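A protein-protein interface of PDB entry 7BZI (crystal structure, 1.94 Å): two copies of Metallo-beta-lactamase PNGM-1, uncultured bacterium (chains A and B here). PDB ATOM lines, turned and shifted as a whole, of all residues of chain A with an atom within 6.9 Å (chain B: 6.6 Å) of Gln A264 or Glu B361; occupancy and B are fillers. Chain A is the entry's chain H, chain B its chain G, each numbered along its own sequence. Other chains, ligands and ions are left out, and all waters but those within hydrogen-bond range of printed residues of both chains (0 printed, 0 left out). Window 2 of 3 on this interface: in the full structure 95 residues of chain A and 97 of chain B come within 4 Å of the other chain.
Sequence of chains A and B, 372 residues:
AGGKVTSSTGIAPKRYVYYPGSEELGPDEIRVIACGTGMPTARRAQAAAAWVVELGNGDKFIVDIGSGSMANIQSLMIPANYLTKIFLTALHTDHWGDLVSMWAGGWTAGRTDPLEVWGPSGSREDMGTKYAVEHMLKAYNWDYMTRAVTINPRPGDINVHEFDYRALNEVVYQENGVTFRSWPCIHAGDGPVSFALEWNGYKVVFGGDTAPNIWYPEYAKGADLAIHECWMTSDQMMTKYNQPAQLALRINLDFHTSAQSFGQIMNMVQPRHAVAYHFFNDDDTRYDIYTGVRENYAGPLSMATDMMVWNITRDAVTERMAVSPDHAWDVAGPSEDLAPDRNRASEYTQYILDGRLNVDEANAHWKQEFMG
N of Leu B357 sits at hydrogen-bond distance from O of Pro A212 (2.9 Å). O of Asn B358 is in hydrogen-bond range of NE2 of Gln A264 (3.1 Å). OE1 of Glu B361 lies close to OE1 of Gln A264 (2.9 Å). OD1 of Asn B363 is in hydrogen-bond range of OG of Ser A258, 2.6 Å away. ND2 of Asn B363 sits at hydrogen-bond distance from OG of Ser A261 (2.9 Å).
ND2 of Asn B358 sits at hydrogen-bond distance from OD2 of Asp B360, 2.9 Å away. The backbone carbonyl oxygen (O) of Val B359 is in hydrogen-bond range of the side-chain amide nitrogen (ND2) of Asn B363. OG of Ser A258 lies close to N of Gln A260, 3.2 Å away. The side-chain hydroxyl (OG) of Ser A258 sits at hydrogen-bond distance from the backbone NH (N) of Ser A261 (2.7 Å). The side-chain amide nitrogen (NE2) of Gln A260 lies within hydrogen-bond range of the side-chain carboxylate (OE1) of Glu A295, 3.1 Å away. The side-chain amide nitrogen (ND2) of Asn A296 sits at hydrogen-bond distance from the backbone carbonyl oxygen (O) of Gln A260, at 3.2 Å.
Val B359 touches Pro A212. Gln A260 touches Ala B362 (CB to O, 3.4 Å). Gln A260 touches Asn B363 (CB to OD1, 3.8 Å). OG of Ser A261 touches CB of Val B359, at 3.5 Å. Gln A264 touches Leu B357 (NE2 to CD2, 3.6 Å). OE1 of Gln A264 touches CA of Val B359 (3.3 Å). Gln A264 touches Ala B362 (OE1 to CB, 3.1 Å). His B365 touches Glu A295 (ND1 to OE2, 3.9 Å). Ala B362 touches Asn A296.
Printed residues of chain B within 4 Å of Gln A264: Leu B357, Asn B358, Val B359, Glu B361 and Ala B362. Glu B361 touches one residue of chain A. Printed residues of chain B within 4 Å of Glu A295: His B365. Of the printed residues of chain A, Val B359 touches Pro A212 (3.5 Å), Ser A261 (3.5 Å) and Gln A264 (3.3 Å). Ala A259 touches none of the printed residues of chain B. Met A268 touches none of the printed residues of chain B. The nearest residue of chain A that does not touch Glu B361 is Asn A296 (6.1 Å).
Hydrophobic or aromatic side chains of chain B within 4 Å of the printed part of chain A: Leu B357, Val B359, Ala B362 and His B365. Of the 19 printed residues of chain A, 7 touch a printed residue of chain B. Hydrophobic or aromatic side chains of chain A that line the printed part of chain B: Pro A212. Among the printed residues, 14 pairs touch across the chains. Among the printed residues, no Asp or Glu carboxylate lies within 4 Å of a Lys or Arg side-chain nitrogen of the other chain.
No position is printed for both chains.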
ATOM      1  N   PRO A 212       6.255  -7.174  23.852  1.00  0.00           N
ATOM      2  CA  PRO A 212       7.367  -8.111  23.704  1.00  0.00           C
ATOM      3  C   PRO A 212       7.825  -8.612  25.081  1.00  0.00           C
ATOM      4  O   PRO A 212       7.963  -7.811  25.997  1.00  0.00           O
ATOM      5  CB  PRO A 212       8.476  -7.313  23.013  1.00  0.00           C
ATOM      6  CG  PRO A 212       7.777  -6.085  22.436  1.00  0.00           C
ATOM      7  CD  PRO A 212       6.536  -5.855  23.272  1.00  0.00           C
ATOM      8  N   PRO A 217      10.385 -15.733  23.058  1.00  0.00           N
ATOM      9  CA  PRO A 217      11.614 -15.991  22.294  1.00  0.00           C
ATOM     10  C   PRO A 217      12.305 -17.291  22.732  1.00  0.00           C
ATOM     11  O   PRO A 217      12.785 -18.016  21.872  1.00  0.00           O
ATOM     12  CB  PRO A 217      12.485 -14.755  22.560  1.00  0.00           C
ATOM     13  CG  PRO A 217      11.482 -13.677  22.947  1.00  0.00           C
ATOM     14  CD  PRO A 217      10.410 -14.421  23.722  1.00  0.00           C
ATOM     15  N   SER A 258       5.004  -4.235  18.028  1.00  0.00           N
ATOM     16  CA  SER A 258       5.292  -3.574  16.727  1.00  0.00           C
ATOM     17  C   SER A 258       5.716  -4.630  15.718  1.00  0.00           C
ATOM     18  O   SER A 258       6.291  -5.658  16.137  1.00  0.00           O
ATOM     19  CB  SER A 258       6.400  -2.552  16.844  1.00  0.00           C
ATOM     20  OG  SER A 258       7.669  -3.210  16.969  1.00  0.00           O
ATOM     21  N   ALA A 259       5.536  -4.339  14.431  1.00  0.00           N
ATOM     22  CA  ALA A 259       6.045  -5.185  13.334  1.00  0.00           C
ATOM     23  C   ALA A 259       7.549  -5.392  13.535  1.00  0.00           C
ATOM     24  O   ALA A 259       8.075  -6.500  13.239  1.00  0.00           O
ATOM     25  CB  ALA A 259       5.730  -4.528  12.015  1.00  0.00           C
ATOM     26  N   GLN A 260       8.226  -4.346  14.023  1.00  0.00           N
ATOM     27  CA  GLN A 260       9.704  -4.329  14.219  1.00  0.00           C
ATOM     28  C   GLN A 260      10.077  -5.302  15.351  1.00  0.00           C
ATOM     29  O   GLN A 260      10.978  -6.170  15.134  1.00  0.00           O
ATOM     30  CB  GLN A 260      10.157  -2.885  14.477  1.00  0.00           C
ATOM     31  CG  GLN A 260      10.211  -2.021  13.220  1.00  0.00           C
ATOM     32  CD  GLN A 260       8.937  -1.276  12.884  1.00  0.00           C
ATOM     33  OE1 GLN A 260       7.938  -1.298  13.610  1.00  0.00           O
ATOM     34  NE2 GLN A 260       8.981  -0.584  11.759  1.00  0.00           N
ATOM     35  N   SER A 261       9.395  -5.188  16.500  1.00  0.00           N
ATOM     36  CA  SER A 261       9.502  -6.146  17.634  1.00  0.00           C
ATOM     37  C   SER A 261       9.227  -7.576  17.143  1.00  0.00           C
ATOM     38  O   SER A 261      10.056  -8.473  17.419  1.00  0.00           O
ATOM     39  CB  SER A 261       8.582  -5.745  18.739  1.00  0.00           C
ATOM     40  OG  SER A 261       9.018  -4.538  19.351  1.00  0.00           O
ATOM     41  N   PHE A 262       8.150  -7.771  16.370  1.00  0.00           N
ATOM     42  CA  PHE A 262       7.775  -9.081  15.760  1.00  0.00           C
ATOM     43  C   PHE A 262       8.993  -9.645  15.027  1.00  0.00           C
ATOM     44  O   PHE A 262       9.363 -10.805  15.221  1.00  0.00           O
ATOM     45  CB  PHE A 262       6.564  -8.927  14.832  1.00  0.00           C
ATOM     46  CG  PHE A 262       6.166 -10.181  14.107  1.00  0.00           C
ATOM     47  CD1 PHE A 262       6.879 -10.614  13.002  1.00  0.00           C
ATOM     48  CD2 PHE A 262       5.084 -10.938  14.537  1.00  0.00           C
ATOM     49  CE1 PHE A 262       6.534 -11.781  12.338  1.00  0.00           C
ATOM     50  CE2 PHE A 262       4.745 -12.109  13.879  1.00  0.00           C
ATOM     51  CZ  PHE A 262       5.457 -12.519  12.773  1.00  0.00           C
ATOM     52  N   GLY A 263       9.628  -8.822  14.199  1.00  0.00           N
ATOM     53  CA  GLY A 263      10.831  -9.246  13.468  1.00  0.00           C
ATOM     54  C   GLY A 263      11.953  -9.630  14.417  1.00  0.00           C
ATOM     55  O   GLY A 263      12.517 -10.738  14.258  1.00  0.00           O
ATOM     56  N   GLN A 264      12.273  -8.762  15.380  1.00  0.00           N
ATOM     57  CA  GLN A 264      13.291  -9.065  16.431  1.00  0.00           C
ATOM     58  C   GLN A 264      12.959 -10.442  17.027  1.00  0.00           C
ATOM     59  O   GLN A 264      13.818 -11.365  16.940  1.00  0.00           O
ATOM     60  CB  GLN A 264      13.326  -7.964  17.492  1.00  0.00           C
ATOM     61  CG  GLN A 264      14.455  -8.122  18.507  1.00  0.00           C
ATOM     62  CD  GLN A 264      14.319  -7.168  19.669  1.00  0.00           C
ATOM     63  OE1 GLN A 264      13.958  -5.998  19.506  1.00  0.00           O
ATOM     64  NE2 GLN A 264      14.615  -7.666  20.863  1.00  0.00           N
ATOM     65  N   ILE A 265      11.711 -10.620  17.480  1.00  0.00           N
ATOM     66  CA  ILE A 265      11.246 -11.860  18.177  1.00  0.00           C
ATOM     67  C   ILE A 265      11.439 -13.039  17.242  1.00  0.00           C
ATOM     68  O   ILE A 265      11.998 -14.049  17.664  1.00  0.00           O
ATOM     69  CB  ILE A 265       9.786 -11.740  18.639  1.00  0.00           C
ATOM     70  CG1 ILE A 265       9.677 -10.807  19.848  1.00  0.00           C
ATOM     71  CG2 ILE A 265       9.203 -13.109  18.930  1.00  0.00           C
ATOM     72  CD1 ILE A 265       8.306 -10.201  20.052  1.00  0.00           C
ATOM     73  N   MET A 266      10.996 -12.915  15.999  1.00  0.00           N
ATOM     74  CA  MET A 266      11.113 -14.041  15.047  1.00  0.00           C
ATOM     75  C   MET A 266      12.578 -14.226  14.642  1.00  0.00           C
ATOM     76  O   MET A 266      12.961 -15.361  14.387  1.00  0.00           O
ATOM     77  CB  MET A 266      10.222 -13.824  13.823  1.00  0.00           C
ATOM     78  CG  MET A 266       8.740 -13.902  14.173  1.00  0.00           C
ATOM     79  SD  MET A 266       8.274 -15.439  14.973  1.00  0.00           S
ATOM     80  CE  MET A 266       6.651 -14.919  15.531  1.00  0.00           C
ATOM     81  N   ASN A 267      13.389 -13.177  14.614  1.00  0.00           N
ATOM     82  CA  ASN A 267      14.849 -13.376  14.392  1.00  0.00           C
ATOM     83  C   ASN A 267      15.391 -14.274  15.523  1.00  0.00           C
ATOM     84  O   ASN A 267      16.086 -15.271  15.212  1.00  0.00           O
ATOM     85  CB  ASN A 267      15.613 -12.057  14.221  1.00  0.00           C
ATOM     86  CG  ASN A 267      17.060 -12.295  13.831  1.00  0.00           C
ATOM     87  OD1 ASN A 267      17.345 -12.971  12.838  1.00  0.00           O
ATOM     88  ND2 ASN A 267      17.975 -11.788  14.639  1.00  0.00           N
ATOM     89  N   MET A 268      15.011 -14.004  16.777  1.00  0.00           N
ATOM     90  CA  MET A 268      15.453 -14.794  17.965  1.00  0.00           C
ATOM     91  C   MET A 268      14.914 -16.229  17.883  1.00  0.00           C
ATOM     92  O   MET A 268      15.692 -17.165  18.130  1.00  0.00           O
ATOM     93  CB  MET A 268      14.992 -14.147  19.272  1.00  0.00           C
ATOM     94  CG  MET A 268      15.484 -12.718  19.456  1.00  0.00           C
ATOM     95  SD  MET A 268      14.664 -11.822  20.813  1.00  0.00           S
ATOM     96  CE  MET A 268      15.416 -12.674  22.202  1.00  0.00           C
ATOM     97  N   VAL A 269      13.639 -16.412  17.519  1.00  0.00           N
ATOM     98  CA  VAL A 269      12.952 -17.741  17.503  1.00  0.00           C
ATOM     99  C   VAL A 269      13.512 -18.632  16.387  1.00  0.00           C
ATOM    100  O   VAL A 269      13.604 -19.836  16.623  1.00  0.00           O
ATOM    101  CB  VAL A 269      11.424 -17.564  17.385  1.00  0.00           C
ATOM    102  CG1 VAL A 269      10.693 -18.880  17.126  1.00  0.00           C
ATOM    103  CG2 VAL A 269      10.867 -16.888  18.629  1.00  0.00           C
ATOM    104  N   GLY A 292       8.224  -3.333   8.132  1.00  0.00           N
ATOM    105  CA  GLY A 292       8.631  -3.306   9.555  1.00  0.00           C
ATOM    106  C   GLY A 292       9.165  -4.650  10.021  1.00  0.00           C
ATOM    107  O   GLY A 292      10.238  -4.684  10.646  1.00  0.00           O
ATOM    108  N   VAL A 293       8.456  -5.739   9.723  1.00  0.00           N
ATOM    109  CA  VAL A 293       8.919  -7.097  10.091  1.00  0.00           C
ATOM    110  C   VAL A 293      10.272  -7.334   9.428  1.00  0.00           C
ATOM    111  O   VAL A 293      11.186  -7.792  10.137  1.00  0.00           O
ATOM    112  CB  VAL A 293       7.898  -8.184   9.715  1.00  0.00           C
ATOM    113  CG1 VAL A 293       8.477  -9.584   9.847  1.00  0.00           C
ATOM    114  CG2 VAL A 293       6.640  -8.057  10.555  1.00  0.00           C
ATOM    115  N   GLU A 295      12.659  -5.570   8.498  1.00  0.00           N
ATOM    116  CA  GLU A 295      13.803  -4.845   9.117  1.00  0.00           C
ATOM    117  C   GLU A 295      14.675  -5.830   9.904  1.00  0.00           C
ATOM    118  O   GLU A 295      15.899  -5.667   9.843  1.00  0.00           O
ATOM    119  CB  GLU A 295      13.366  -3.716  10.053  1.00  0.00           C
ATOM    120  CG  GLU A 295      12.843  -2.494   9.325  1.00  0.00           C
ATOM    121  CD  GLU A 295      12.614  -1.316  10.257  1.00  0.00           C
ATOM    122  OE1 GLU A 295      11.598  -0.615  10.117  1.00  0.00           O
ATOM    123  OE2 GLU A 295      13.448  -1.121  11.140  1.00  0.00           O
ATOM    124  N   ASN A 296      14.077  -6.811  10.592  1.00  0.00           N
ATOM    125  CA  ASN A 296      14.783  -7.660  11.589  1.00  0.00           C
ATOM    126  C   ASN A 296      14.637  -9.150  11.261  1.00  0.00           C
ATOM    127  O   ASN A 296      15.553  -9.910  11.633  1.00  0.00           O
ATOM    128  CB  ASN A 296      14.337  -7.262  12.998  1.00  0.00           C
ATOM    129  CG  ASN A 296      14.592  -5.790  13.223  1.00  0.00           C
ATOM    130  OD1 ASN A 296      15.623  -5.296  12.804  1.00  0.00           O
ATOM    131  ND2 ASN A 296      13.666  -5.075  13.827  1.00  0.00           N
ATOM    132  N   TYR A 297      13.568  -9.570  10.578  1.00  0.00           N
ATOM    133  CA  TYR A 297      13.315 -10.996  10.243  1.00  0.00           C
ATOM    134  C   TYR A 297      13.381 -11.208   8.721  1.00  0.00           C
ATOM    135  O   TYR A 297      12.670 -10.503   7.986  1.00  0.00           O
ATOM    136  CB  TYR A 297      11.977 -11.446  10.845  1.00  0.00           C
ATOM    137  CG  TYR A 297      11.635 -12.885  10.542  1.00  0.00           C
ATOM    138  CD1 TYR A 297      12.454 -13.914  10.967  1.00  0.00           C
ATOM    139  CD2 TYR A 297      10.519 -13.222   9.794  1.00  0.00           C
ATOM    140  CE1 TYR A 297      12.177 -15.234  10.658  1.00  0.00           C
ATOM    141  CE2 TYR A 297      10.230 -14.538   9.475  1.00  0.00           C
ATOM    142  CZ  TYR A 297      11.054 -15.554   9.917  1.00  0.00           C
ATOM    143  OH  TYR A 297      10.768 -16.855   9.618  1.00  0.00           O
ATOM    144  N   LEU B 357      10.540  -7.767  27.291  1.00  0.00           N
ATOM    145  CA  LEU B 357      11.776  -7.887  26.473  1.00  0.00           C
ATOM    146  C   LEU B 357      12.282  -6.485  26.108  1.00  0.00           C
ATOM    147  O   LEU B 357      11.447  -5.603  25.866  1.00  0.00           O
ATOM    148  CB  LEU B 357      11.479  -8.686  25.203  1.00  0.00           C
ATOM    149  CG  LEU B 357      12.684  -8.912  24.291  1.00  0.00           C
ATOM    150  CD1 LEU B 357      13.660  -9.895  24.927  1.00  0.00           C
ATOM    151  CD2 LEU B 357      12.249  -9.399  22.914  1.00  0.00           C
ATOM    152  N   ASN B 358      13.602  -6.284  26.074  1.00  0.00           N
ATOM    153  CA  ASN B 358      14.201  -5.026  25.558  1.00  0.00           C
ATOM    154  C   ASN B 358      14.083  -5.045  24.029  1.00  0.00           C
ATOM    155  O   ASN B 358      14.681  -5.949  23.406  1.00  0.00           O
ATOM    156  CB  ASN B 358      15.663  -4.821  25.962  1.00  0.00           C
ATOM    157  CG  ASN B 358      16.185  -3.497  25.441  1.00  0.00           C
ATOM    158  OD1 ASN B 358      16.727  -3.431  24.340  1.00  0.00           O
ATOM    159  ND2 ASN B 358      15.941  -2.424  26.178  1.00  0.00           N
ATOM    160  N   VAL B 359      13.341  -4.095  23.459  1.00  0.00           N
ATOM    161  CA  VAL B 359      13.144  -3.973  21.979  1.00  0.00           C
ATOM    162  C   VAL B 359      13.554  -2.570  21.510  1.00  0.00           C
ATOM    163  O   VAL B 359      13.202  -2.228  20.367  1.00  0.00           O
ATOM    164  CB  VAL B 359      11.691  -4.298  21.565  1.00  0.00           C
ATOM    165  CG1 VAL B 359      11.333  -5.746  21.874  1.00  0.00           C
ATOM    166  CG2 VAL B 359      10.680  -3.338  22.182  1.00  0.00           C
ATOM    167  N   ASP B 360      14.268  -1.804  22.347  1.00  0.00           N
ATOM    168  CA  ASP B 360      14.709  -0.409  22.067  1.00  0.00           C
ATOM    169  C   ASP B 360      15.329  -0.337  20.663  1.00  0.00           C
ATOM    170  O   ASP B 360      14.914   0.556  19.880  1.00  0.00           O
ATOM    171  CB  ASP B 360      15.725   0.074  23.104  1.00  0.00           C
ATOM    172  CG  ASP B 360      15.184   0.256  24.514  1.00  0.00           C
ATOM    173  OD1 ASP B 360      13.949   0.264  24.674  1.00  0.00           O
ATOM    174  OD2 ASP B 360      16.013   0.406  25.443  1.00  0.00           O
ATOM    175  N   GLU B 361      16.243  -1.271  20.358  1.00  0.00           N
ATOM    176  CA  GLU B 361      17.132  -1.248  19.156  1.00  0.00           C
ATOM    177  C   GLU B 361      16.258  -1.329  17.895  1.00  0.00           C
ATOM    178  O   GLU B 361      16.328  -0.398  17.048  1.00  0.00           O
ATOM    179  CB  GLU B 361      18.170  -2.390  19.112  1.00  0.00           C
ATOM    180  CG  GLU B 361      18.373  -3.201  20.398  1.00  0.00           C
ATOM    181  CD  GLU B 361      17.677  -4.562  20.482  1.00  0.00           C
ATOM    182  OE1 GLU B 361      16.463  -4.646  20.147  1.00  0.00           O
ATOM    183  OE2 GLU B 361      18.352  -5.549  20.887  1.00  0.00           O
ATOM    184  N   ALA B 362      15.454  -2.399  17.809  1.00  0.00           N
ATOM    185  CA  ALA B 362      14.608  -2.798  16.658  1.00  0.00           C
ATOM    186  C   ALA B 362      13.595  -1.692  16.328  1.00  0.00           C
ATOM    187  O   ALA B 362      13.216  -1.553  15.154  1.00  0.00           O
ATOM    188  CB  ALA B 362      13.936  -4.118  16.981  1.00  0.00           C
ATOM    189  N   ASN B 363      13.197  -0.905  17.324  1.00  0.00           N
ATOM    190  CA  ASN B 363      12.129   0.120  17.186  1.00  0.00           C
ATOM    191  C   ASN B 363      12.718   1.544  17.086  1.00  0.00           C
ATOM    192  O   ASN B 363      11.924   2.481  16.865  1.00  0.00           O
ATOM    193  CB  ASN B 363      11.113  -0.009  18.327  1.00  0.00           C
ATOM    194  CG  ASN B 363      10.266  -1.265  18.227  1.00  0.00           C
ATOM    195  OD1 ASN B 363       9.120  -1.208  17.782  1.00  0.00           O
ATOM    196  ND2 ASN B 363      10.814  -2.396  18.648  1.00  0.00           N
ATOM    197  N   ALA B 364      14.037   1.736  17.238  1.00  0.00           N
ATOM    198  CA  ALA B 364      14.664   3.085  17.303  1.00  0.00           C
ATOM    199  C   ALA B 364      14.638   3.748  15.914  1.00  0.00           C
ATOM    200  O   ALA B 364      14.270   4.937  15.851  1.00  0.00           O
ATOM    201  CB  ALA B 364      16.061   3.010  17.876  1.00  0.00           C
ATOM    202  N   HIS B 365      14.959   3.010  14.842  1.00  0.00           N
ATOM    203  CA  HIS B 365      14.919   3.502  13.432  1.00  0.00           C
ATOM    204  C   HIS B 365      13.556   4.155  13.110  1.00  0.00           C
ATOM    205  O   HIS B 365      13.558   5.348  12.748  1.00  0.00           O
ATOM    206  CB  HIS B 365      15.309   2.375  12.457  1.00  0.00           C
ATOM    207  CG  HIS B 365      15.468   2.813  11.038  1.00  0.00           C
ATOM    208  ND1 HIS B 365      15.688   1.909  10.008  1.00  0.00           N
ATOM    209  CD2 HIS B 365      15.423   4.039  10.465  1.00  0.00           C
ATOM    210  CE1 HIS B 365      15.779   2.562   8.865  1.00  0.00           C
ATOM    211  NE2 HIS B 365      15.622   3.872   9.120  1.00  0.00           N
